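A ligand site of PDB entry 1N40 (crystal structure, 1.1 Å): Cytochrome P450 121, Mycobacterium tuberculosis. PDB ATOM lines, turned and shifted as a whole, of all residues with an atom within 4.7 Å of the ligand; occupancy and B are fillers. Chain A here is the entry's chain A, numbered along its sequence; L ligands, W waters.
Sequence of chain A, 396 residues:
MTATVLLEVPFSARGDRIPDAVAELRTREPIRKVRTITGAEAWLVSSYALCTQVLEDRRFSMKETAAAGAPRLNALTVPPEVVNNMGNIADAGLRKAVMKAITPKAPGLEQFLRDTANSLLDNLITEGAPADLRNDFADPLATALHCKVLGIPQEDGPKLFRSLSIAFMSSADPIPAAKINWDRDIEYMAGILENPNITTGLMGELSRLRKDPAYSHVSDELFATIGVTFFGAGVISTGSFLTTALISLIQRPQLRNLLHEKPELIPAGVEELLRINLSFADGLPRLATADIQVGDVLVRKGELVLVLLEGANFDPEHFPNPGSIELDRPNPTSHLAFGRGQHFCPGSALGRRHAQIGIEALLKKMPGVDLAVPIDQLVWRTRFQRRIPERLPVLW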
ATOM      1  N   MET A  62     -23.818 -21.922 -15.450  1.00  0.00           N
ATOM      2  CA  MET A  62     -22.998 -22.458 -14.355  1.00  0.00           C
ATOM      3  C   MET A  62     -22.595 -23.896 -14.685  1.00  0.00           C
ATOM      4  O   MET A  62     -21.420 -24.265 -14.558  1.00  0.00           O
ATOM      5  CB  MET A  62     -23.746 -22.378 -13.016  1.00  0.00           C
ATOM      6  CG  MET A  62     -23.051 -23.192 -11.888  1.00  0.00           C
ATOM      7  SD  MET A  62     -24.014 -23.209 -10.362  1.00  0.00           S
ATOM      8  CE  MET A  62     -23.702 -21.565  -9.772  1.00  0.00           C
ATOM      9  N   MET A  86     -27.379 -27.874  -7.532  1.00  0.00           N
ATOM     10  CA  MET A  86     -28.772 -27.432  -7.371  1.00  0.00           C
ATOM     11  C   MET A  86     -29.703 -27.979  -8.453  1.00  0.00           C
ATOM     12  O   MET A  86     -30.807 -28.386  -8.170  1.00  0.00           O
ATOM     13  CB  MET A  86     -28.835 -25.925  -7.236  1.00  0.00           C
ATOM     14  CG  MET A  86     -28.389 -25.589  -5.856  1.00  0.00           C
ATOM     15  SD  MET A  86     -29.577 -25.781  -4.504  1.00  0.00           S
ATOM     16  CE  MET A  86     -30.636 -24.272  -4.444  1.00  0.00           C
ATOM     17  N   ILE A 102     -33.436 -25.301   5.347  1.00  0.00           N
ATOM     18  CA  ILE A 102     -32.296 -24.385   5.579  1.00  0.00           C
ATOM     19  C   ILE A 102     -32.723 -22.931   5.721  1.00  0.00           C
ATOM     20  O   ILE A 102     -31.894 -22.018   5.663  1.00  0.00           O
ATOM     21  CB  ILE A 102     -31.190 -24.555   4.507  1.00  0.00           C
ATOM     22  CG1 ILE A 102     -31.650 -24.064   3.141  1.00  0.00           C
ATOM     23  CG2 ILE A 102     -30.698 -26.016   4.491  1.00  0.00           C
ATOM     24  CD1 ILE A 102     -30.579 -24.009   2.085  1.00  0.00           C
ATOM     25  N   HIS A 146     -24.745 -24.682  11.476  1.00  0.00           N
ATOM     26  CA  HIS A 146     -24.933 -25.651  10.396  1.00  0.00           C
ATOM     27  C   HIS A 146     -25.035 -27.076  10.897  1.00  0.00           C
ATOM     28  O   HIS A 146     -25.749 -27.867  10.303  1.00  0.00           O
ATOM     29  CB  HIS A 146     -23.912 -25.462   9.291  1.00  0.00           C
ATOM     30  CG  HIS A 146     -24.189 -24.244   8.473  1.00  0.00           C
ATOM     31  ND1 HIS A 146     -23.899 -22.967   8.901  1.00  0.00           N
ATOM     32  CD2 HIS A 146     -24.876 -24.099   7.327  1.00  0.00           C
ATOM     33  CE1 HIS A 146     -24.394 -22.110   8.021  1.00  0.00           C
ATOM     34  NE2 HIS A 146     -24.993 -22.763   7.053  1.00  0.00           N
ATOM     35  N   THR A 229     -22.079 -30.425   0.584  1.00  0.00           N
ATOM     36  CA  THR A 229     -22.116 -29.141  -0.126  1.00  0.00           C
ATOM     37  C   THR A 229     -22.815 -28.055   0.669  1.00  0.00           C
ATOM     38  O   THR A 229     -22.352 -26.939   0.677  1.00  0.00           O
ATOM     39  CB  THR A 229     -22.735 -29.322  -1.540  1.00  0.00           C
ATOM     40  OG1 THR A 229     -22.966 -28.081  -2.207  1.00  0.00           O
ATOM     41  CG2 THR A 229     -24.027 -29.859  -1.482  1.00  0.00           C
ATOM     42  N   PHE A 230     -23.929 -28.376   1.315  1.00  0.00           N
ATOM     43  CA  PHE A 230     -24.656 -27.366   2.064  1.00  0.00           C
ATOM     44  C   PHE A 230     -23.933 -27.017   3.372  1.00  0.00           C
ATOM     45  O   PHE A 230     -23.882 -25.842   3.728  1.00  0.00           O
ATOM     46  CB  PHE A 230     -26.131 -27.768   2.298  1.00  0.00           C
ATOM     47  CG  PHE A 230     -26.994 -27.440   1.104  1.00  0.00           C
ATOM     48  CD1 PHE A 230     -26.792 -28.073  -0.119  1.00  0.00           C
ATOM     49  CD2 PHE A 230     -27.924 -26.408   1.126  1.00  0.00           C
ATOM     50  CE1 PHE A 230     -27.546 -27.743  -1.237  1.00  0.00           C
ATOM     51  CE2 PHE A 230     -28.673 -26.064  -0.008  1.00  0.00           C
ATOM     52  CZ  PHE A 230     -28.482 -26.753  -1.168  1.00  0.00           C
ATOM     53  N   ALA A 233     -20.759 -24.871   1.947  1.00  0.00           N
ATOM     54  CA  ALA A 233     -21.155 -23.569   1.414  1.00  0.00           C
ATOM     55  C   ALA A 233     -21.697 -22.692   2.525  1.00  0.00           C
ATOM     56  O   ALA A 233     -21.365 -21.519   2.622  1.00  0.00           O
ATOM     57  CB  ALA A 233     -22.180 -23.678   0.285  1.00  0.00           C
ATOM     58  N   GLY A 234     -22.540 -23.249   3.375  1.00  0.00           N
ATOM     59  CA  GLY A 234     -23.160 -22.421   4.393  1.00  0.00           C
ATOM     60  C   GLY A 234     -22.139 -21.962   5.426  1.00  0.00           C
ATOM     61  O   GLY A 234     -22.119 -20.784   5.810  1.00  0.00           O
ATOM     62  N   SER A 237     -19.579 -19.508   3.922  1.00  0.00           N
ATOM     63  CA  SER A 237     -20.161 -18.243   3.499  1.00  0.00           C
ATOM     64  C   SER A 237     -20.575 -17.366   4.678  1.00  0.00           C
ATOM     65  O   SER A 237     -20.316 -16.178   4.676  1.00  0.00           O
ATOM     66  CB  SER A 237     -21.337 -18.450   2.552  1.00  0.00           C
ATOM     67  OG  SER A 237     -20.957 -19.188   1.386  1.00  0.00           O
ATOM     68  N   THR A 238     -21.241 -17.984   5.649  1.00  0.00           N
ATOM     69  CA  THR A 238     -21.677 -17.254   6.839  1.00  0.00           C
ATOM     70  C   THR A 238     -20.505 -16.876   7.733  1.00  0.00           C
ATOM     71  O   THR A 238     -20.451 -15.758   8.239  1.00  0.00           O
ATOM     72  CB  THR A 238     -22.749 -18.013   7.638  1.00  0.00           C
ATOM     73  OG1 THR A 238     -22.248 -19.269   8.098  1.00  0.00           O
ATOM     74  CG2 THR A 238     -24.012 -18.197   6.838  1.00  0.00           C
ATOM     75  N   PHE A 241     -18.569 -14.091   5.766  1.00  0.00           N
ATOM     76  CA  PHE A 241     -19.327 -12.849   5.677  1.00  0.00           C
ATOM     77  C   PHE A 241     -19.369 -12.169   7.058  1.00  0.00           C
ATOM     78  O   PHE A 241     -19.121 -10.966   7.154  1.00  0.00           O
ATOM     79  CB  PHE A 241     -20.762 -13.064   5.172  1.00  0.00           C
ATOM     80  CG  PHE A 241     -21.572 -11.832   5.320  1.00  0.00           C
ATOM     81  CD1 PHE A 241     -21.213 -10.675   4.620  1.00  0.00           C
ATOM     82  CD2 PHE A 241     -22.585 -11.751   6.249  1.00  0.00           C
ATOM     83  CE1 PHE A 241     -21.863  -9.474   4.869  1.00  0.00           C
ATOM     84  CE2 PHE A 241     -23.282 -10.552   6.464  1.00  0.00           C
ATOM     85  CZ  PHE A 241     -22.903  -9.419   5.792  1.00  0.00           C
ATOM     86  N   LEU A 274     -23.991  -6.556   3.773  1.00  0.00           N
ATOM     87  CA  LEU A 274     -24.046  -7.460   2.631  1.00  0.00           C
ATOM     88  C   LEU A 274     -23.706  -6.729   1.334  1.00  0.00           C
ATOM     89  O   LEU A 274     -22.890  -7.187   0.549  1.00  0.00           O
ATOM     90  CB  LEU A 274     -25.456  -8.133   2.525  1.00  0.00           C
ATOM     91  CG  LEU A 274     -25.685  -9.254   3.517  1.00  0.00           C
ATOM     92  CD1 LEU A 274     -27.170  -9.520   3.693  1.00  0.00           C
ATOM     93  CD2 LEU A 274     -24.964 -10.555   3.103  1.00  0.00           C
ATOM     94  N   PHE A 280     -16.637 -12.599  -1.462  1.00  0.00           N
ATOM     95  CA  PHE A 280     -16.336 -13.442  -2.631  1.00  0.00           C
ATOM     96  C   PHE A 280     -15.049 -12.927  -3.279  1.00  0.00           C
ATOM     97  O   PHE A 280     -14.956 -11.778  -3.705  1.00  0.00           O
ATOM     98  CB  PHE A 280     -17.477 -13.490  -3.638  1.00  0.00           C
ATOM     99  CG  PHE A 280     -18.506 -14.538  -3.301  1.00  0.00           C
ATOM    100  CD1 PHE A 280     -19.240 -14.466  -2.130  1.00  0.00           C
ATOM    101  CD2 PHE A 280     -18.675 -15.636  -4.103  1.00  0.00           C
ATOM    102  CE1 PHE A 280     -20.168 -15.475  -1.796  1.00  0.00           C
ATOM    103  CE2 PHE A 280     -19.615 -16.637  -3.771  1.00  0.00           C
ATOM    104  CZ  PHE A 280     -20.351 -16.536  -2.613  1.00  0.00           C
ATOM    105  N   LEU A 284     -18.239 -14.488 -10.070  1.00  0.00           N
ATOM    106  CA  LEU A 284     -18.989 -15.730 -10.253  1.00  0.00           C
ATOM    107  C   LEU A 284     -18.803 -16.219 -11.679  1.00  0.00           C
ATOM    108  O   LEU A 284     -19.052 -15.460 -12.622  1.00  0.00           O
ATOM    109  CB  LEU A 284     -20.471 -15.520  -9.988  1.00  0.00           C
ATOM    110  CG  LEU A 284     -20.841 -14.954  -8.603  1.00  0.00           C
ATOM    111  CD1 LEU A 284     -22.359 -14.847  -8.520  1.00  0.00           C
ATOM    112  CD2 LEU A 284     -20.272 -15.805  -7.477  1.00  0.00           C
ATOM    113  N   ARG A 286     -19.320 -18.204 -15.267  1.00  0.00           N
ATOM    114  CA  ARG A 286     -20.347 -18.740 -16.169  1.00  0.00           C
ATOM    115  C   ARG A 286     -19.690 -18.996 -17.523  1.00  0.00           C
ATOM    116  O   ARG A 286     -18.762 -18.279 -17.910  1.00  0.00           O
ATOM    117  CB  ARG A 286     -21.454 -17.710 -16.403  1.00  0.00           C
ATOM    118  CG  ARG A 286     -22.250 -17.319 -15.175  1.00  0.00           C
ATOM    119  CD  ARG A 286     -23.088 -18.473 -14.648  1.00  0.00           C
ATOM    120  NE  ARG A 286     -24.018 -18.088 -13.602  1.00  0.00           N
ATOM    121  CZ  ARG A 286     -23.811 -18.160 -12.270  1.00  0.00           C
ATOM    122  NH1 ARG A 286     -22.644 -18.549 -11.778  1.00  0.00           N
ATOM    123  NH2 ARG A 286     -24.781 -17.828 -11.456  1.00  0.00           N
ATOM    124  N   LEU A 309     -19.092  -9.311  -8.119  1.00  0.00           N
ATOM    125  CA  LEU A 309     -20.184  -8.887  -7.257  1.00  0.00           C
ATOM    126  C   LEU A 309     -19.964  -7.488  -6.716  1.00  0.00           C
ATOM    127  O   LEU A 309     -20.927  -6.694  -6.661  1.00  0.00           O
ATOM    128  CB  LEU A 309     -20.434  -9.870  -6.118  1.00  0.00           C
ATOM    129  CG  LEU A 309     -20.858 -11.282  -6.595  1.00  0.00           C
ATOM    130  CD1 LEU A 309     -21.131 -12.156  -5.387  1.00  0.00           C
ATOM    131  CD2 LEU A 309     -22.081 -11.235  -7.486  1.00  0.00           C
ATOM    132  N   LEU A 336     -26.375  -7.706  -5.082  1.00  0.00           N
ATOM    133  CA  LEU A 336     -26.098  -9.030  -5.631  1.00  0.00           C
ATOM    134  C   LEU A 336     -25.277  -9.909  -4.675  1.00  0.00           C
ATOM    135  O   LEU A 336     -24.633 -10.860  -5.102  1.00  0.00           O
ATOM    136  CB  LEU A 336     -25.374  -8.945  -6.990  1.00  0.00           C
ATOM    137  CG  LEU A 336     -26.059  -8.138  -8.069  1.00  0.00           C
ATOM    138  CD1 LEU A 336     -25.378  -8.333  -9.408  1.00  0.00           C
ATOM    139  CD2 LEU A 336     -27.512  -8.337  -8.166  1.00  0.00           C
ATOM    140  N   ALA A 337     -25.296  -9.608  -3.376  1.00  0.00           N
ATOM    141  CA  ALA A 337     -24.487 -10.414  -2.442  1.00  0.00           C
ATOM    142  C   ALA A 337     -24.855 -11.875  -2.422  1.00  0.00           C
ATOM    143  O   ALA A 337     -23.997 -12.714  -2.127  1.00  0.00           O
ATOM    144  CB  ALA A 337     -24.566  -9.872  -1.037  1.00  0.00           C
ATOM    145  N   PHE A 338     -26.119 -12.200  -2.706  1.00  0.00           N
ATOM    146  CA  PHE A 338     -26.622 -13.568  -2.769  1.00  0.00           C
ATOM    147  C   PHE A 338     -26.756 -14.066  -4.197  1.00  0.00           C
ATOM    148  O   PHE A 338     -27.444 -15.073  -4.473  1.00  0.00           O
ATOM    149  CB  PHE A 338     -27.954 -13.716  -2.015  1.00  0.00           C
ATOM    150  CG  PHE A 338     -27.816 -13.468  -0.516  1.00  0.00           C
ATOM    151  CD1 PHE A 338     -27.053 -14.319   0.273  1.00  0.00           C
ATOM    152  CD2 PHE A 338     -28.510 -12.440   0.105  1.00  0.00           C
ATOM    153  CE1 PHE A 338     -26.983 -14.134   1.630  1.00  0.00           C
ATOM    154  CE2 PHE A 338     -28.422 -12.258   1.453  1.00  0.00           C
ATOM    155  CZ  PHE A 338     -27.666 -13.100   2.223  1.00  0.00           C
ATOM    156  N   GLY A 339     -26.147 -13.371  -5.141  1.00  0.00           N
ATOM    157  CA  GLY A 339     -26.353 -13.676  -6.529  1.00  0.00           C
ATOM    158  C   GLY A 339     -27.692 -13.175  -7.043  1.00  0.00           C
ATOM    159  O   GLY A 339     -28.294 -12.250  -6.489  1.00  0.00           O
ATOM    160  N   GLN A 342     -31.158 -17.864 -11.689  1.00  0.00           N
ATOM    161  CA  GLN A 342     -31.311 -19.292 -11.483  1.00  0.00           C
ATOM    162  C   GLN A 342     -30.578 -19.805 -10.241  1.00  0.00           C
ATOM    163  O   GLN A 342     -31.043 -20.722  -9.593  1.00  0.00           O
ATOM    164  CB  GLN A 342     -30.781 -20.024 -12.735  1.00  0.00           C
ATOM    165  CG  GLN A 342     -30.874 -21.522 -12.703  1.00  0.00           C
ATOM    166  CD  GLN A 342     -32.274 -22.089 -12.862  1.00  0.00           C
ATOM    167  OE1 GLN A 342     -32.461 -23.300 -12.739  1.00  0.00           O
ATOM    168  NE2 GLN A 342     -33.225 -21.275 -13.189  1.00  0.00           N
ATOM    169  N   HIS A 343     -29.404 -19.263  -9.964  1.00  0.00           N
ATOM    170  CA  HIS A 343     -28.550 -19.754  -8.904  1.00  0.00           C
ATOM    171  C   HIS A 343     -28.514 -18.897  -7.641  1.00  0.00           C
ATOM    172  O   HIS A 343     -27.623 -19.036  -6.812  1.00  0.00           O
ATOM    173  CB  HIS A 343     -27.155 -20.004  -9.465  1.00  0.00           C
ATOM    174  CG  HIS A 343     -27.175 -21.061 -10.513  1.00  0.00           C
ATOM    175  ND1 HIS A 343     -27.421 -22.372 -10.223  1.00  0.00           N
ATOM    176  CD2 HIS A 343     -27.038 -20.991 -11.861  1.00  0.00           C
ATOM    177  CE1 HIS A 343     -27.435 -23.060 -11.349  1.00  0.00           C
ATOM    178  NE2 HIS A 343     -27.221 -22.251 -12.349  1.00  0.00           N
ATOM    179  N   PHE A 344     -29.540 -18.054  -7.464  1.00  0.00           N
ATOM    180  CA  PHE A 344     -29.669 -17.236  -6.271  1.00  0.00           C
ATOM    181  C   PHE A 344     -29.513 -18.114  -5.031  1.00  0.00           C
ATOM    182  O   PHE A 344     -30.077 -19.205  -4.948  1.00  0.00           O
ATOM    183  CB  PHE A 344     -31.048 -16.547  -6.265  1.00  0.00           C
ATOM    184  CG  PHE A 344     -31.284 -15.646  -5.084  1.00  0.00           C
ATOM    185  CD1 PHE A 344     -30.806 -14.368  -5.083  1.00  0.00           C
ATOM    186  CD2 PHE A 344     -31.904 -16.106  -3.948  1.00  0.00           C
ATOM    187  CE1 PHE A 344     -30.995 -13.537  -3.979  1.00  0.00           C
ATOM    188  CE2 PHE A 344     -32.086 -15.268  -2.854  1.00  0.00           C
ATOM    189  CZ  PHE A 344     -31.624 -14.010  -2.886  1.00  0.00           C
ATOM    190  N   CYS A 345     -28.763 -17.626  -4.051  1.00  0.00           N
ATOM    191  CA  CYS A 345     -28.408 -18.383  -2.860  1.00  0.00           C
ATOM    192  C   CYS A 345     -29.666 -18.972  -2.181  1.00  0.00           C
ATOM    193  O   CYS A 345     -30.509 -18.177  -1.746  1.00  0.00           O
ATOM    194  CB  CYS A 345     -27.711 -17.484  -1.877  1.00  0.00           C
ATOM    195  SG  CYS A 345     -27.192 -18.372  -0.378  1.00  0.00           S
ATOM    196  N   PRO A 346     -29.736 -20.273  -1.965  1.00  0.00           N
ATOM    197  CA  PRO A 346     -30.877 -20.861  -1.243  1.00  0.00           C
ATOM    198  C   PRO A 346     -30.786 -20.672   0.265  1.00  0.00           C
ATOM    199  O   PRO A 346     -31.743 -20.995   0.967  1.00  0.00           O
ATOM    200  CB  PRO A 346     -30.781 -22.337  -1.614  1.00  0.00           C
ATOM    201  CG  PRO A 346     -29.296 -22.554  -1.797  1.00  0.00           C
ATOM    202  CD  PRO A 346     -28.813 -21.305  -2.461  1.00  0.00           C
ATOM    203  N   GLY A 347     -29.653 -20.190   0.766  1.00  0.00           N
ATOM    204  CA  GLY A 347     -29.432 -19.965   2.183  1.00  0.00           C
ATOM    205  C   GLY A 347     -29.543 -18.495   2.598  1.00  0.00           C
ATOM    206  O   GLY A 347     -29.118 -18.164   3.702  1.00  0.00           O
ATOM    207  N   LEU A 350     -31.163 -17.602   6.048  1.00  0.00           N
ATOM    208  CA  LEU A 350     -30.321 -18.105   7.111  1.00  0.00           C
ATOM    209  C   LEU A 350     -29.045 -17.283   7.274  1.00  0.00           C
ATOM    210  O   LEU A 350     -28.609 -17.017   8.393  1.00  0.00           O
ATOM    211  CB  LEU A 350     -30.026 -19.588   6.871  1.00  0.00           C
ATOM    212  CG  LEU A 350     -29.282 -20.323   7.966  1.00  0.00           C
ATOM    213  CD1 LEU A 350     -30.113 -20.411   9.233  1.00  0.00           C
ATOM    214  CD2 LEU A 350     -28.872 -21.704   7.512  1.00  0.00           C
ATOM    215  N   GLY A 351     -28.435 -16.915   6.161  1.00  0.00           N
ATOM    216  CA  GLY A 351     -27.242 -16.105   6.213  1.00  0.00           C
ATOM    217  C   GLY A 351     -27.510 -14.732   6.845  1.00  0.00           C
ATOM    218  O   GLY A 351     -26.724 -14.262   7.685  1.00  0.00           O
HETATM  219  C1  LIG L   1     -25.136 -19.781  -3.883  1.00  0.00           C
HETATM  220  C2  LIG L   1     -23.662 -16.029  -1.307  1.00  0.00           C
HETATM  221  C3  LIG L   1     -25.016 -18.351   2.727  1.00  0.00           C
HETATM  222  C4  LIG L   1     -25.724 -22.314   0.153  1.00  0.00           C
HETATM  223  C5  LIG L   1     -24.728 -18.524  -3.530  1.00  0.00           C
HETATM  224  C6  LIG L   1     -24.351 -17.484  -4.489  1.00  0.00           C
HETATM  225  C7  LIG L   1     -23.865 -16.491  -3.766  1.00  0.00           C
HETATM  226  C8  LIG L   1     -24.007 -16.838  -2.359  1.00  0.00           C
HETATM  227  C9  LIG L   1     -23.279 -15.188  -4.279  1.00  0.00           C
HETATM  228  C10 LIG L   1     -24.483 -17.597  -6.008  1.00  0.00           C
HETATM  229  C11 LIG L   1     -23.362 -18.294  -6.711  1.00  0.00           C
HETATM  230  C12 LIG L   1     -23.481 -18.253  -8.213  1.00  0.00           C
HETATM  231  O1  LIG L   1     -24.532 -17.819  -8.753  1.00  0.00           O
HETATM  232  O2  LIG L   1     -22.457 -18.627  -8.891  1.00  0.00           O
HETATM  233  C13 LIG L   1     -23.854 -16.357   0.029  1.00  0.00           C
HETATM  234  C14 LIG L   1     -23.614 -15.465   1.146  1.00  0.00           C
HETATM  235  C15 LIG L   1     -24.006 -16.113   2.276  1.00  0.00           C
HETATM  236  C16 LIG L   1     -24.468 -17.393   1.883  1.00  0.00           C
HETATM  237  C17 LIG L   1     -23.002 -14.088   1.002  1.00  0.00           C
HETATM  238  C18 LIG L   1     -23.981 -15.639   3.711  1.00  0.00           C
HETATM  239  C19 LIG L   1     -24.140 -14.378   4.091  1.00  0.00           C
HETATM  240  C20 LIG L   1     -25.421 -19.630   2.363  1.00  0.00           C
HETATM  241  C21 LIG L   1     -25.952 -20.654   3.266  1.00  0.00           C
HETATM  242  C22 LIG L   1     -26.091 -21.755   2.559  1.00  0.00           C
HETATM  243  C23 LIG L   1     -25.724 -21.461   1.208  1.00  0.00           C
HETATM  244  C24 LIG L   1     -26.253 -20.437   4.744  1.00  0.00           C
HETATM  245  C25 LIG L   1     -26.608 -23.115   2.971  1.00  0.00           C
HETATM  246  C26 LIG L   1     -26.912 -23.509   4.190  1.00  0.00           C
HETATM  247  C27 LIG L   1     -25.565 -22.025  -1.172  1.00  0.00           C
HETATM  248  C28 LIG L   1     -25.625 -22.986  -2.237  1.00  0.00           C
HETATM  249  C29 LIG L   1     -25.503 -22.203  -3.469  1.00  0.00           C
HETATM  250  C30 LIG L   1     -25.312 -20.858  -3.058  1.00  0.00           C
HETATM  251  C31 LIG L   1     -25.817 -24.473  -2.132  1.00  0.00           C
HETATM  252  C32 LIG L   1     -25.520 -22.727  -4.871  1.00  0.00           C
HETATM  253  C33 LIG L   1     -26.838 -22.449  -5.535  1.00  0.00           C
HETATM  254  C34 LIG L   1     -26.806 -22.880  -7.000  1.00  0.00           C
HETATM  255  O3  LIG L   1     -27.891 -22.720  -7.575  1.00  0.00           O
HETATM  256  O4  LIG L   1     -25.784 -23.367  -7.528  1.00  0.00           O
HETATM  257  N1  LIG L   1     -24.504 -18.114  -2.229  1.00  0.00           N
HETATM  258  N2  LIG L   1     -24.341 -17.535   0.514  1.00  0.00           N
HETATM  259  N3  LIG L   1     -25.318 -20.153   1.110  1.00  0.00           N
HETATM  260  N4  LIG L   1     -25.297 -20.774  -1.675  1.00  0.00           N
HETATM  261 FE1  LIG L   1     -25.050 -19.080  -0.563  1.00  0.00          FE
HETATM  262  O   HOH W   1     -30.039 -21.748  -6.152  1.00  0.00           O
HETATM  263  O   HOH W   2     -23.089 -23.779  -6.812  1.00  0.00           O
HETATM  264  O   HOH W   3     -30.459 -23.559  -9.281  1.00  0.00           O
HETATM  265  O   HOH W   4     -21.845 -19.838  -3.321  1.00  0.00           O
HETATM  266  O   HOH W   5     -25.427 -25.866  -8.534  1.00  0.00           O
HETATM  267  O   HOH W   6     -26.705 -16.219  -8.736  1.00  0.00           O
HETATM  268  O   HOH W   7     -20.436 -20.068  -7.958  1.00  0.00           O
HETATM  269  O   HOH W   8     -26.096 -26.825  -4.622  1.00  0.00           O
HETATM  270  O   HOH W   9     -22.931 -19.821  -0.594  1.00  0.00           O
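Water W5 lies within hydrogen-bond range of an oxygen (O4) of the ligand, the backbone NH of Met 86 and the side-chain sulfur of Met 62.
Water W1 bridges an oxygen (O3) of the ligand (2.8 Å) and the backbone carbonyl oxygen (O) of Phe 344 (2.8 Å).
Water W2 lies within hydrogen-bond range of an oxygen (O4) of the ligand (2.8 Å) and the side-chain sulfur of Met 62 (3.7 Å).
Water W3 lies within hydrogen-bond range of O of Gln 342, O3 of the ligand and ND1 of His 343.
An oxygen (O4) of the ligand sits close to the side-chain sulfur (SD) of Met 62.
CG of Met 86 touches C34 of the ligand, 3.3 Å away.
His 146 touches the ligand (NE2 to C24, 3.5 Å).
Phe 230 touches the ligand.
Ala 233 touches the ligand.
Gly 234 touches the ligand.
Ser 237 touches the ligand (CB to C16, 3.4 Å).
CG2 of Thr 238 touches C24 of the ligand, at 3.8 Å.
Phe 241 touches the ligand.
Phe 280 touches the ligand.
Leu 284 touches the ligand (CD1 to C12, 3.6 Å).
Leu 309 touches the ligand (CD1 to C9, 3.9 Å).
Ala 337 touches the ligand.
Phe 338 touches the ligand (CE1 to C15, 3.6 Å).
Gly 339 touches the ligand.
Pro 346 touches the ligand.
Gly 347 touches the ligand.
Of the 28 residues printed, 20 come within 4 Å of the ligand.
N of Cys 345 lies within hydrogen-bond range of O of Phe 338 (2.9 Å).
SG of Cys 345 lies close to N of Gly 347, 3.3 Å away.
A ring nitrogen (ND1) of His 343 lies within hydrogen-bond range of the side-chain sulfur (SD) of Met 62, 3.5 Å away.
O of Ala 233 is in hydrogen-bond range of OG of Ser 237.
O of Gly 234 is in hydrogen-bond range of OG1 of Thr 238 (2.7 Å).
SG of Cys 345 binds FE1 of the ligand (2.3 Å).
ND1 of His 343 is in hydrogen-bond range of O3 of the ligand (2.7 Å).
O1 of the ligand lies within salt-bridge range of NH2 of Arg 286 (2.7 Å).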
